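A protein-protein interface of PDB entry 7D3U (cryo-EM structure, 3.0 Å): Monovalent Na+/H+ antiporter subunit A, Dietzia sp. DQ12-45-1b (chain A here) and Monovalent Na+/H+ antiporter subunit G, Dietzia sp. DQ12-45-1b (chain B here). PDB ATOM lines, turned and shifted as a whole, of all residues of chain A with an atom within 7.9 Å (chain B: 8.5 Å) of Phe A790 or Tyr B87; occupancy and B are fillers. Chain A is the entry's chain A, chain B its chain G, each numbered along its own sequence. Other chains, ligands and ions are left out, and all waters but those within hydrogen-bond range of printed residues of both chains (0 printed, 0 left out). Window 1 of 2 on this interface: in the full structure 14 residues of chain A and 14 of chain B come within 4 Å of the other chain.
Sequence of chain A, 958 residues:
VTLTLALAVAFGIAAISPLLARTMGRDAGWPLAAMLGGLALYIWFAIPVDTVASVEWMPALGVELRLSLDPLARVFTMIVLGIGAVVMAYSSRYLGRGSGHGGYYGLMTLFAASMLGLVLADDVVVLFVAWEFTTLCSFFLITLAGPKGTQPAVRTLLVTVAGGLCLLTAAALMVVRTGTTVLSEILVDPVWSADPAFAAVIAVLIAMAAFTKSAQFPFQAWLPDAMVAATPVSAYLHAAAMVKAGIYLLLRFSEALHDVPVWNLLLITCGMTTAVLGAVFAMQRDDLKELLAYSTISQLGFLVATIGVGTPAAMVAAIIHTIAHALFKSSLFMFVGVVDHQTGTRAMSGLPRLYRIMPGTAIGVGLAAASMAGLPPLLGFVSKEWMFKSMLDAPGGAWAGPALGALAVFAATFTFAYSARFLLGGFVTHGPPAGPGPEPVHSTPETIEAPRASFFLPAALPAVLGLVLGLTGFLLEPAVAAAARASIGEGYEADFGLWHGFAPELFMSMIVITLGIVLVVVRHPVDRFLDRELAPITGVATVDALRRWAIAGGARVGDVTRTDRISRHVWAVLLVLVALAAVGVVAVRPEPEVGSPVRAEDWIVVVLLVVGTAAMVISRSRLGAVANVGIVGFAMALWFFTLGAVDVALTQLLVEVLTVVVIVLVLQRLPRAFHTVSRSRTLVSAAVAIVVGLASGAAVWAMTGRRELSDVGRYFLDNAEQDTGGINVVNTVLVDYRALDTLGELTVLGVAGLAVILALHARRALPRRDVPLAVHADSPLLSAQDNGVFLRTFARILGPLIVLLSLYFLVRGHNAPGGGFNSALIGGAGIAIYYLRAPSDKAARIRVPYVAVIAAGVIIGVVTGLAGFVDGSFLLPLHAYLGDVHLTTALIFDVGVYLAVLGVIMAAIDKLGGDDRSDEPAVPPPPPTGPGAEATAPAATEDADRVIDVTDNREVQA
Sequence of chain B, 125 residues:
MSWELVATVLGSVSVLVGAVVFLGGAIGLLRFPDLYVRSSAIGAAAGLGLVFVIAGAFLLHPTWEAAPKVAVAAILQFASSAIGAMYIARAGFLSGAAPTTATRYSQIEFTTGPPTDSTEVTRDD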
ATOM      1  N   LEU A 781      38.835  20.888  26.753  1.00  0.00           N
ATOM      2  CA  LEU A 781      37.603  20.265  27.231  1.00  0.00           C
ATOM      3  C   LEU A 781      37.620  20.068  28.741  1.00  0.00           C
ATOM      4  O   LEU A 781      36.811  19.312  29.283  1.00  0.00           O
ATOM      5  CB  LEU A 781      37.315  18.936  26.520  1.00  0.00           C
ATOM      6  CG  LEU A 781      37.479  18.940  24.996  1.00  0.00           C
ATOM      7  CD1 LEU A 781      36.877  17.705  24.376  1.00  0.00           C
ATOM      8  CD2 LEU A 781      36.847  20.168  24.389  1.00  0.00           C
ATOM      9  N   ALA A 784      36.787  24.228  33.547  1.00  0.00           N
ATOM     10  CA  ALA A 784      35.401  24.679  33.435  1.00  0.00           C
ATOM     11  C   ALA A 784      35.271  26.195  33.395  1.00  0.00           C
ATOM     12  O   ALA A 784      34.379  26.719  32.722  1.00  0.00           O
ATOM     13  CB  ALA A 784      34.583  24.116  34.596  1.00  0.00           C
ATOM     14  N   GLN A 785      36.147  26.918  34.098  1.00  0.00           N
ATOM     15  CA  GLN A 785      36.092  28.375  34.054  1.00  0.00           C
ATOM     16  C   GLN A 785      36.293  28.891  32.636  1.00  0.00           C
ATOM     17  O   GLN A 785      35.646  29.860  32.222  1.00  0.00           O
ATOM     18  CB  GLN A 785      37.139  28.968  34.994  1.00  0.00           C
ATOM     19  CG  GLN A 785      36.655  30.186  35.762  1.00  0.00           C
ATOM     20  CD  GLN A 785      36.381  31.371  34.859  1.00  0.00           C
ATOM     21  OE1 GLN A 785      37.105  31.609  33.894  1.00  0.00           O
ATOM     22  NE2 GLN A 785      35.329  32.121  35.168  1.00  0.00           N
ATOM     23  N   ASP A 786      37.182  28.255  31.878  1.00  0.00           N
ATOM     24  CA  ASP A 786      37.455  28.647  30.504  1.00  0.00           C
ATOM     25  C   ASP A 786      36.595  27.910  29.489  1.00  0.00           C
ATOM     26  O   ASP A 786      36.544  28.327  28.328  1.00  0.00           O
ATOM     27  CB  ASP A 786      38.933  28.413  30.176  1.00  0.00           C
ATOM     28  CG  ASP A 786      39.761  29.672  30.301  1.00  0.00           C
ATOM     29  OD1 ASP A 786      39.171  30.749  30.529  1.00  0.00           O
ATOM     30  OD2 ASP A 786      41.000  29.586  30.171  1.00  0.00           O
ATOM     31  N   ASN A 787      35.916  26.837  29.892  1.00  0.00           N
ATOM     32  CA  ASN A 787      35.153  26.013  28.967  1.00  0.00           C
ATOM     33  C   ASN A 787      33.648  26.190  29.088  1.00  0.00           C
ATOM     34  O   ASN A 787      32.912  25.663  28.248  1.00  0.00           O
ATOM     35  CB  ASN A 787      35.503  24.534  29.165  1.00  0.00           C
ATOM     36  CG  ASN A 787      35.224  23.704  27.935  1.00  0.00           C
ATOM     37  OD1 ASN A 787      35.058  24.238  26.842  1.00  0.00           O
ATOM     38  ND2 ASN A 787      35.175  22.392  28.106  1.00  0.00           N
ATOM     39  N   GLY A 788      33.170  26.902  30.104  1.00  0.00           N
ATOM     40  CA  GLY A 788      31.756  27.186  30.216  1.00  0.00           C
ATOM     41  C   GLY A 788      31.417  28.525  29.602  1.00  0.00           C
ATOM     42  O   GLY A 788      30.413  29.149  29.958  1.00  0.00           O
ATOM     43  N   VAL A 789      32.263  28.976  28.673  1.00  0.00           N
ATOM     44  CA  VAL A 789      32.065  30.275  28.038  1.00  0.00           C
ATOM     45  C   VAL A 789      30.783  30.289  27.221  1.00  0.00           C
ATOM     46  O   VAL A 789      30.163  31.344  27.042  1.00  0.00           O
ATOM     47  CB  VAL A 789      33.292  30.638  27.180  1.00  0.00           C
ATOM     48  CG1 VAL A 789      33.376  29.746  25.955  1.00  0.00           C
ATOM     49  CG2 VAL A 789      33.243  32.094  26.773  1.00  0.00           C
ATOM     50  N   PHE A 790      30.358  29.130  26.718  1.00  0.00           N
ATOM     51  CA  PHE A 790      29.150  29.078  25.905  1.00  0.00           C
ATOM     52  C   PHE A 790      27.916  29.381  26.740  1.00  0.00           C
ATOM     53  O   PHE A 790      27.064  30.181  26.339  1.00  0.00           O
ATOM     54  CB  PHE A 790      29.030  27.712  25.233  1.00  0.00           C
ATOM     55  CG  PHE A 790      30.298  27.250  24.583  1.00  0.00           C
ATOM     56  CD1 PHE A 790      30.913  28.019  23.617  1.00  0.00           C
ATOM     57  CD2 PHE A 790      30.871  26.042  24.932  1.00  0.00           C
ATOM     58  CE1 PHE A 790      32.078  27.598  23.016  1.00  0.00           C
ATOM     59  CE2 PHE A 790      32.034  25.616  24.333  1.00  0.00           C
ATOM     60  CZ  PHE A 790      32.637  26.396  23.374  1.00  0.00           C
ATOM     61  N   LEU A 791      27.801  28.754  27.910  1.00  0.00           N
ATOM     62  CA  LEU A 791      26.660  29.028  28.771  1.00  0.00           C
ATOM     63  C   LEU A 791      26.787  30.368  29.480  1.00  0.00           C
ATOM     64  O   LEU A 791      25.775  31.042  29.699  1.00  0.00           O
ATOM     65  CB  LEU A 791      26.484  27.908  29.794  1.00  0.00           C
ATOM     66  CG  LEU A 791      25.166  27.961  30.566  1.00  0.00           C
ATOM     67  CD1 LEU A 791      24.001  28.111  29.608  1.00  0.00           C
ATOM     68  CD2 LEU A 791      24.998  26.722  31.424  1.00  0.00           C
ATOM     69  N   ARG A 792      28.006  30.776  29.840  1.00  0.00           N
ATOM     70  CA  ARG A 792      28.180  32.052  30.523  1.00  0.00           C
ATOM     71  C   ARG A 792      27.829  33.235  29.634  1.00  0.00           C
ATOM     72  O   ARG A 792      27.586  34.331  30.150  1.00  0.00           O
ATOM     73  CB  ARG A 792      29.615  32.190  31.034  1.00  0.00           C
ATOM     74  CG  ARG A 792      29.894  31.390  32.296  1.00  0.00           C
ATOM     75  CD  ARG A 792      31.196  31.807  32.958  1.00  0.00           C
ATOM     76  NE  ARG A 792      32.368  31.324  32.235  1.00  0.00           N
ATOM     77  CZ  ARG A 792      33.077  32.061  31.389  1.00  0.00           C
ATOM     78  NH1 ARG A 792      32.737  33.320  31.160  1.00  0.00           N
ATOM     79  NH2 ARG A 792      34.131  31.541  30.775  1.00  0.00           N
ATOM     80  N   THR A 793      27.800  33.046  28.316  1.00  0.00           N
ATOM     81  CA  THR A 793      27.403  34.101  27.393  1.00  0.00           C
ATOM     82  C   THR A 793      25.935  34.006  27.001  1.00  0.00           C
ATOM     83  O   THR A 793      25.233  35.020  26.983  1.00  0.00           O
ATOM     84  CB  THR A 793      28.278  34.070  26.137  1.00  0.00           C
ATOM     85  OG1 THR A 793      29.625  34.406  26.487  1.00  0.00           O
ATOM     86  CG2 THR A 793      27.768  35.077  25.121  1.00  0.00           C
ATOM     87  N   PHE A 794      25.455  32.804  26.679  1.00  0.00           N
ATOM     88  CA  PHE A 794      24.037  32.641  26.383  1.00  0.00           C
ATOM     89  C   PHE A 794      23.175  33.034  27.571  1.00  0.00           C
ATOM     90  O   PHE A 794      22.031  33.466  27.393  1.00  0.00           O
ATOM     91  CB  PHE A 794      23.744  31.202  25.972  1.00  0.00           C
ATOM     92  CG  PHE A 794      22.357  30.994  25.439  1.00  0.00           C
ATOM     93  CD1 PHE A 794      21.787  31.917  24.582  1.00  0.00           C
ATOM     94  CD2 PHE A 794      21.625  29.874  25.791  1.00  0.00           C
ATOM     95  CE1 PHE A 794      20.511  31.729  24.088  1.00  0.00           C
ATOM     96  CE2 PHE A 794      20.349  29.681  25.299  1.00  0.00           C
ATOM     97  CZ  PHE A 794      19.792  30.608  24.447  1.00  0.00           C
ATOM     98  N   ALA A 795      23.700  32.898  28.789  1.00  0.00           N
ATOM     99  CA  ALA A 795      22.967  33.365  29.956  1.00  0.00           C
ATOM    100  C   ALA A 795      22.857  34.882  29.995  1.00  0.00           C
ATOM    101  O   ALA A 795      21.909  35.398  30.588  1.00  0.00           O
ATOM    102  CB  ALA A 795      23.625  32.859  31.236  1.00  0.00           C
ATOM    103  N   ARG A 796      23.779  35.603  29.353  1.00  0.00           N
ATOM    104  CA  ARG A 796      23.672  37.057  29.300  1.00  0.00           C
ATOM    105  C   ARG A 796      22.434  37.513  28.541  1.00  0.00           C
ATOM    106  O   ARG A 796      22.001  38.657  28.715  1.00  0.00           O
ATOM    107  CB  ARG A 796      24.922  37.657  28.658  1.00  0.00           C
ATOM    108  CG  ARG A 796      26.113  37.761  29.591  1.00  0.00           C
ATOM    109  CD  ARG A 796      27.346  38.220  28.838  1.00  0.00           C
ATOM    110  NE  ARG A 796      27.024  39.255  27.860  1.00  0.00           N
ATOM    111  CZ  ARG A 796      27.881  39.730  26.964  1.00  0.00           C
ATOM    112  NH1 ARG A 796      29.119  39.260  26.914  1.00  0.00           N
ATOM    113  NH2 ARG A 796      27.500  40.672  26.114  1.00  0.00           N
ATOM    114  N   LEU A 836      23.785  26.146  36.678  1.00  0.00           N
ATOM    115  CA  LEU A 836      24.582  25.483  35.650  1.00  0.00           C
ATOM    116  C   LEU A 836      25.660  26.402  35.090  1.00  0.00           C
ATOM    117  O   LEU A 836      26.676  25.923  34.571  1.00  0.00           O
ATOM    118  CB  LEU A 836      23.679  24.990  34.521  1.00  0.00           C
ATOM    119  CG  LEU A 836      22.603  23.968  34.883  1.00  0.00           C
ATOM    120  CD1 LEU A 836      21.744  23.659  33.673  1.00  0.00           C
ATOM    121  CD2 LEU A 836      23.232  22.703  35.428  1.00  0.00           C
ATOM    122  N   ARG A 837      25.460  27.715  35.182  1.00  0.00           N
ATOM    123  CA  ARG A 837      26.397  28.671  34.605  1.00  0.00           C
ATOM    124  C   ARG A 837      27.671  28.811  35.427  1.00  0.00           C
ATOM    125  O   ARG A 837      28.728  29.126  34.870  1.00  0.00           O
ATOM    126  CB  ARG A 837      25.714  30.032  34.464  1.00  0.00           C
ATOM    127  CG  ARG A 837      26.605  31.138  33.943  1.00  0.00           C
ATOM    128  CD  ARG A 837      25.881  32.463  33.950  1.00  0.00           C
ATOM    129  NE  ARG A 837      25.957  33.118  35.250  1.00  0.00           N
ATOM    130  CZ  ARG A 837      26.777  34.124  35.528  1.00  0.00           C
ATOM    131  NH1 ARG A 837      27.592  34.595  34.596  1.00  0.00           N
ATOM    132  NH2 ARG A 837      26.780  34.663  36.739  1.00  0.00           N
ATOM    133  N   LEU B  35      29.407   9.082  19.025  1.00  0.00           N
ATOM    134  CA  LEU B  35      28.592  10.060  19.732  1.00  0.00           C
ATOM    135  C   LEU B  35      28.801  11.455  19.169  1.00  0.00           C
ATOM    136  O   LEU B  35      27.878  12.276  19.189  1.00  0.00           O
ATOM    137  CB  LEU B  35      28.926  10.046  21.226  1.00  0.00           C
ATOM    138  CG  LEU B  35      28.158  10.968  22.176  1.00  0.00           C
ATOM    139  CD1 LEU B  35      28.070  10.321  23.530  1.00  0.00           C
ATOM    140  CD2 LEU B  35      28.820  12.327  22.311  1.00  0.00           C
ATOM    141  N   SER B  39      26.088  13.939  17.654  1.00  0.00           N
ATOM    142  CA  SER B  39      25.867  15.288  18.163  1.00  0.00           C
ATOM    143  C   SER B  39      26.054  16.329  17.069  1.00  0.00           C
ATOM    144  O   SER B  39      25.332  17.331  17.032  1.00  0.00           O
ATOM    145  CB  SER B  39      26.805  15.566  19.335  1.00  0.00           C
ATOM    146  OG  SER B  39      26.626  14.611  20.364  1.00  0.00           O
ATOM    147  N   ALA B  79      20.089  28.781  19.188  1.00  0.00           N
ATOM    148  CA  ALA B  79      21.166  28.830  20.171  1.00  0.00           C
ATOM    149  C   ALA B  79      21.127  27.627  21.105  1.00  0.00           C
ATOM    150  O   ALA B  79      22.176  27.083  21.470  1.00  0.00           O
ATOM    151  CB  ALA B  79      21.087  30.131  20.968  1.00  0.00           C
ATOM    152  N   SER B  80      19.928  27.176  21.483  1.00  0.00           N
ATOM    153  CA  SER B  80      19.824  26.068  22.422  1.00  0.00           C
ATOM    154  C   SER B  80      20.190  24.747  21.764  1.00  0.00           C
ATOM    155  O   SER B  80      20.877  23.922  22.369  1.00  0.00           O
ATOM    156  CB  SER B  80      18.416  26.012  23.011  1.00  0.00           C
ATOM    157  OG  SER B  80      17.514  25.383  22.121  1.00  0.00           O
ATOM    158  N   SER B  81      19.753  24.528  20.523  1.00  0.00           N
ATOM    159  CA  SER B  81      20.138  23.312  19.823  1.00  0.00           C
ATOM    160  C   SER B  81      21.625  23.283  19.515  1.00  0.00           C
ATOM    161  O   SER B  81      22.191  22.198  19.358  1.00  0.00           O
ATOM    162  CB  SER B  81      19.346  23.166  18.526  1.00  0.00           C
ATOM    163  OG  SER B  81      19.748  22.008  17.819  1.00  0.00           O
ATOM    164  N   ALA B  82      22.270  24.446  19.427  1.00  0.00           N
ATOM    165  CA  ALA B  82      23.723  24.454  19.297  1.00  0.00           C
ATOM    166  C   ALA B  82      24.394  24.114  20.625  1.00  0.00           C
ATOM    167  O   ALA B  82      25.224  23.198  20.702  1.00  0.00           O
ATOM    168  CB  ALA B  82      24.197  25.810  18.785  1.00  0.00           C
ATOM    169  N   ILE B  83      24.026  24.833  21.688  1.00  0.00           N
ATOM    170  CA  ILE B  83      24.757  24.738  22.948  1.00  0.00           C
ATOM    171  C   ILE B  83      24.507  23.398  23.630  1.00  0.00           C
ATOM    172  O   ILE B  83      25.421  22.815  24.225  1.00  0.00           O
ATOM    173  CB  ILE B  83      24.387  25.922  23.855  1.00  0.00           C
ATOM    174  CG1 ILE B  83      24.958  27.210  23.270  1.00  0.00           C
ATOM    175  CG2 ILE B  83      24.910  25.713  25.263  1.00  0.00           C
ATOM    176  CD1 ILE B  83      24.584  28.433  24.037  1.00  0.00           C
ATOM    177  N   GLY B  84      23.273  22.895  23.573  1.00  0.00           N
ATOM    178  CA  GLY B  84      22.990  21.603  24.171  1.00  0.00           C
ATOM    179  C   GLY B  84      23.814  20.494  23.554  1.00  0.00           C
ATOM    180  O   GLY B  84      24.399  19.672  24.261  1.00  0.00           O
ATOM    181  N   ALA B  85      23.883  20.464  22.222  1.00  0.00           N
ATOM    182  CA  ALA B  85      24.693  19.453  21.552  1.00  0.00           C
ATOM    183  C   ALA B  85      26.172  19.642  21.858  1.00  0.00           C
ATOM    184  O   ALA B  85      26.899  18.662  22.056  1.00  0.00           O
ATOM    185  CB  ALA B  85      24.446  19.495  20.046  1.00  0.00           C
ATOM    186  N   MET B  86      26.632  20.896  21.911  1.00  0.00           N
ATOM    187  CA  MET B  86      28.026  21.158  22.254  1.00  0.00           C
ATOM    188  C   MET B  86      28.374  20.575  23.617  1.00  0.00           C
ATOM    189  O   MET B  86      29.367  19.852  23.767  1.00  0.00           O
ATOM    190  CB  MET B  86      28.292  22.663  22.233  1.00  0.00           C
ATOM    191  CG  MET B  86      28.588  23.216  20.859  1.00  0.00           C
ATOM    192  SD  MET B  86      28.011  24.904  20.635  1.00  0.00           S
ATOM    193  CE  MET B  86      28.578  25.647  22.156  1.00  0.00           C
ATOM    194  N   TYR B  87      27.547  20.860  24.623  1.00  0.00           N
ATOM    195  CA  TYR B  87      27.850  20.398  25.970  1.00  0.00           C
ATOM    196  C   TYR B  87      27.648  18.898  26.114  1.00  0.00           C
ATOM    197  O   TYR B  87      28.369  18.256  26.881  1.00  0.00           O
ATOM    198  CB  TYR B  87      27.007  21.153  26.992  1.00  0.00           C
ATOM    199  CG  TYR B  87      27.620  22.467  27.404  1.00  0.00           C
ATOM    200  CD1 TYR B  87      28.949  22.746  27.131  1.00  0.00           C
ATOM    201  CD2 TYR B  87      26.871  23.428  28.063  1.00  0.00           C
ATOM    202  CE1 TYR B  87      29.514  23.943  27.503  1.00  0.00           C
ATOM    203  CE2 TYR B  87      27.428  24.627  28.438  1.00  0.00           C
ATOM    204  CZ  TYR B  87      28.750  24.880  28.155  1.00  0.00           C
ATOM    205  OH  TYR B  87      29.307  26.078  28.529  1.00  0.00           O
ATOM    206  N   ILE B  88      26.694  18.318  25.384  1.00  0.00           N
ATOM    207  CA  ILE B  88      26.532  16.868  25.417  1.00  0.00           C
ATOM    208  C   ILE B  88      27.769  16.186  24.850  1.00  0.00           C
ATOM    209  O   ILE B  88      28.278  15.219  25.425  1.00  0.00           O
ATOM    210  CB  ILE B  88      25.256  16.447  24.667  1.00  0.00           C
ATOM    211  CG1 ILE B  88      24.015  16.825  25.474  1.00  0.00           C
ATOM    212  CG2 ILE B  88      25.267  14.958  24.397  1.00  0.00           C
ATOM    213  CD1 ILE B  88      23.957  16.179  26.828  1.00  0.00           C
ATOM    214  N   ALA B  89      28.284  16.691  23.726  1.00  0.00           N
ATOM    215  CA  ALA B  89      29.493  16.109  23.152  1.00  0.00           C
ATOM    216  C   ALA B  89      30.685  16.277  24.085  1.00  0.00           C
ATOM    217  O   ALA B  89      31.483  15.348  24.259  1.00  0.00           O
ATOM    218  CB  ALA B  89      29.784  16.737  21.792  1.00  0.00           C
ATOM    219  N   ARG B  90      30.822  17.455  24.698  1.00  0.00           N
ATOM    220  CA  ARG B  90      31.943  17.678  25.608  1.00  0.00           C
ATOM    221  C   ARG B  90      31.869  16.745  26.810  1.00  0.00           C
ATOM    222  O   ARG B  90      32.870  16.126  27.191  1.00  0.00           O
ATOM    223  CB  ARG B  90      31.974  19.136  26.061  1.00  0.00           C
ATOM    224  CG  ARG B  90      33.032  19.417  27.106  1.00  0.00           C
ATOM    225  CD  ARG B  90      32.483  20.278  28.220  1.00  0.00           C
ATOM    226  NE  ARG B  90      33.435  20.419  29.315  1.00  0.00           N
ATOM    227  CZ  ARG B  90      33.152  20.993  30.478  1.00  0.00           C
ATOM    228  NH1 ARG B  90      31.940  21.482  30.699  1.00  0.00           N
ATOM    229  NH2 ARG B  90      34.080  21.080  31.420  1.00  0.00           N
ATOM    230  N   ALA B  91      30.689  16.630  27.423  1.00  0.00           N
ATOM    231  CA  ALA B  91      30.534  15.745  28.571  1.00  0.00           C
ATOM    232  C   ALA B  91      30.715  14.284  28.184  1.00  0.00           C
ATOM    233  O   ALA B  91      31.189  13.486  28.998  1.00  0.00           O
ATOM    234  CB  ALA B  91      29.168  15.958  29.218  1.00  0.00           C
ATOM    235  N   GLY B  92      30.347  13.914  26.957  1.00  0.00           N
ATOM    236  CA  GLY B  92      30.612  12.561  26.503  1.00  0.00           C
ATOM    237  C   GLY B  92      32.095  12.296  26.356  1.00  0.00           C
ATOM    238  O   GLY B  92      32.581  11.220  26.715  1.00  0.00           O
ATOM    239  N   PHE B  93      32.836  13.278  25.841  1.00  0.00           N
ATOM    240  CA  PHE B  93      34.288  13.151  25.795  1.00  0.00           C
ATOM    241  C   PHE B  93      34.862  12.997  27.196  1.00  0.00           C
ATOM    242  O   PHE B  93      35.717  12.138  27.440  1.00  0.00           O
ATOM    243  CB  PHE B  93      34.903  14.362  25.095  1.00  0.00           C
ATOM    244  CG  PHE B  93      36.405  14.346  25.066  1.00  0.00           C
ATOM    245  CD1 PHE B  93      37.142  14.839  26.130  1.00  0.00           C
ATOM    246  CD2 PHE B  93      37.080  13.838  23.973  1.00  0.00           C
ATOM    247  CE1 PHE B  93      38.517  14.826  26.103  1.00  0.00           C
ATOM    248  CE2 PHE B  93      38.456  13.823  23.943  1.00  0.00           C
ATOM    249  CZ  PHE B  93      39.174  14.314  25.012  1.00  0.00           C
ATOM    250  N   LEU B  94      34.407  13.832  28.130  1.00  0.00           N
ATOM    251  CA  LEU B  94      34.914  13.758  29.495  1.00  0.00           C
ATOM    252  C   LEU B  94      34.533  12.442  30.159  1.00  0.00           C
ATOM    253  O   LEU B  94      35.359  11.823  30.841  1.00  0.00           O
ATOM    254  CB  LEU B  94      34.400  14.940  30.311  1.00  0.00           C
ATOM    255  CG  LEU B  94      35.042  16.286  29.989  1.00  0.00           C
ATOM    256  CD1 LEU B  94      34.661  17.321  31.030  1.00  0.00           C
ATOM    257  CD2 LEU B  94      36.547  16.141  29.904  1.00  0.00           C
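The guanidinium group (NE) of Arg B90 lies close to the side-chain amide nitrogen (ND2) of Asn A787 (2.9 Å). The backbone NH of Leu A791 sits at hydrogen-bond distance from the side-chain hydroxyl of Tyr B87 (3.1 Å).
Hydrophobic or aromatic side chains of chain A within 4 Å of the printed part of chain B: Leu A781, Phe A790, Leu A791 and Phe A794. Among the printed residues, 12 pairs touch across the chains.
Arg B90 touches Leu A781 (NE to O, 3.6 Å). CD1 of Leu A781 touches CD1 of Phe B93 (3.4 Å). O of Leu A781 touches CD2 of Leu B94 (3.2 Å). Asn A787 touches Tyr B87 (O to OH, 3.6 Å). Tyr B87 touches Gly A788. O of Phe A790 touches CD1 of Ile B83 (3.8 Å). Met B86 touches Phe A790. CE1 of Tyr B87 touches CD2 of Phe A790 (3.6 Å). Ala B79 touches Phe A794 (CB to CE1, 3.6 Å). Phe A794 touches Ile B83.
Of the printed residues of chain B, Asn A787 touches Tyr B87 and Arg B90. Gly A788 touches just one residue of chain B: Tyr B87 (3.2 Å). Phe A790 touches just these residues of chain B: Ile B83 (3.8 Å), Met B86 (3.4 Å) and Tyr B87 (3.6 Å). Ala A795 touches none of the printed residues of chain B. Of chain A, only Asn A787, Gly A788, Phe A790 and Leu A791 come within 4 Å of Tyr B87. Printed residues of chain A within 4 Å of Phe B93: Leu A781 (3.4 Å). The nearest residue of chain A that does not touch Tyr B87 is Val A789 (4.1 Å). The nearest printed residue of chain B that does not touch Asn A787 is Leu B94 (5.9 Å).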
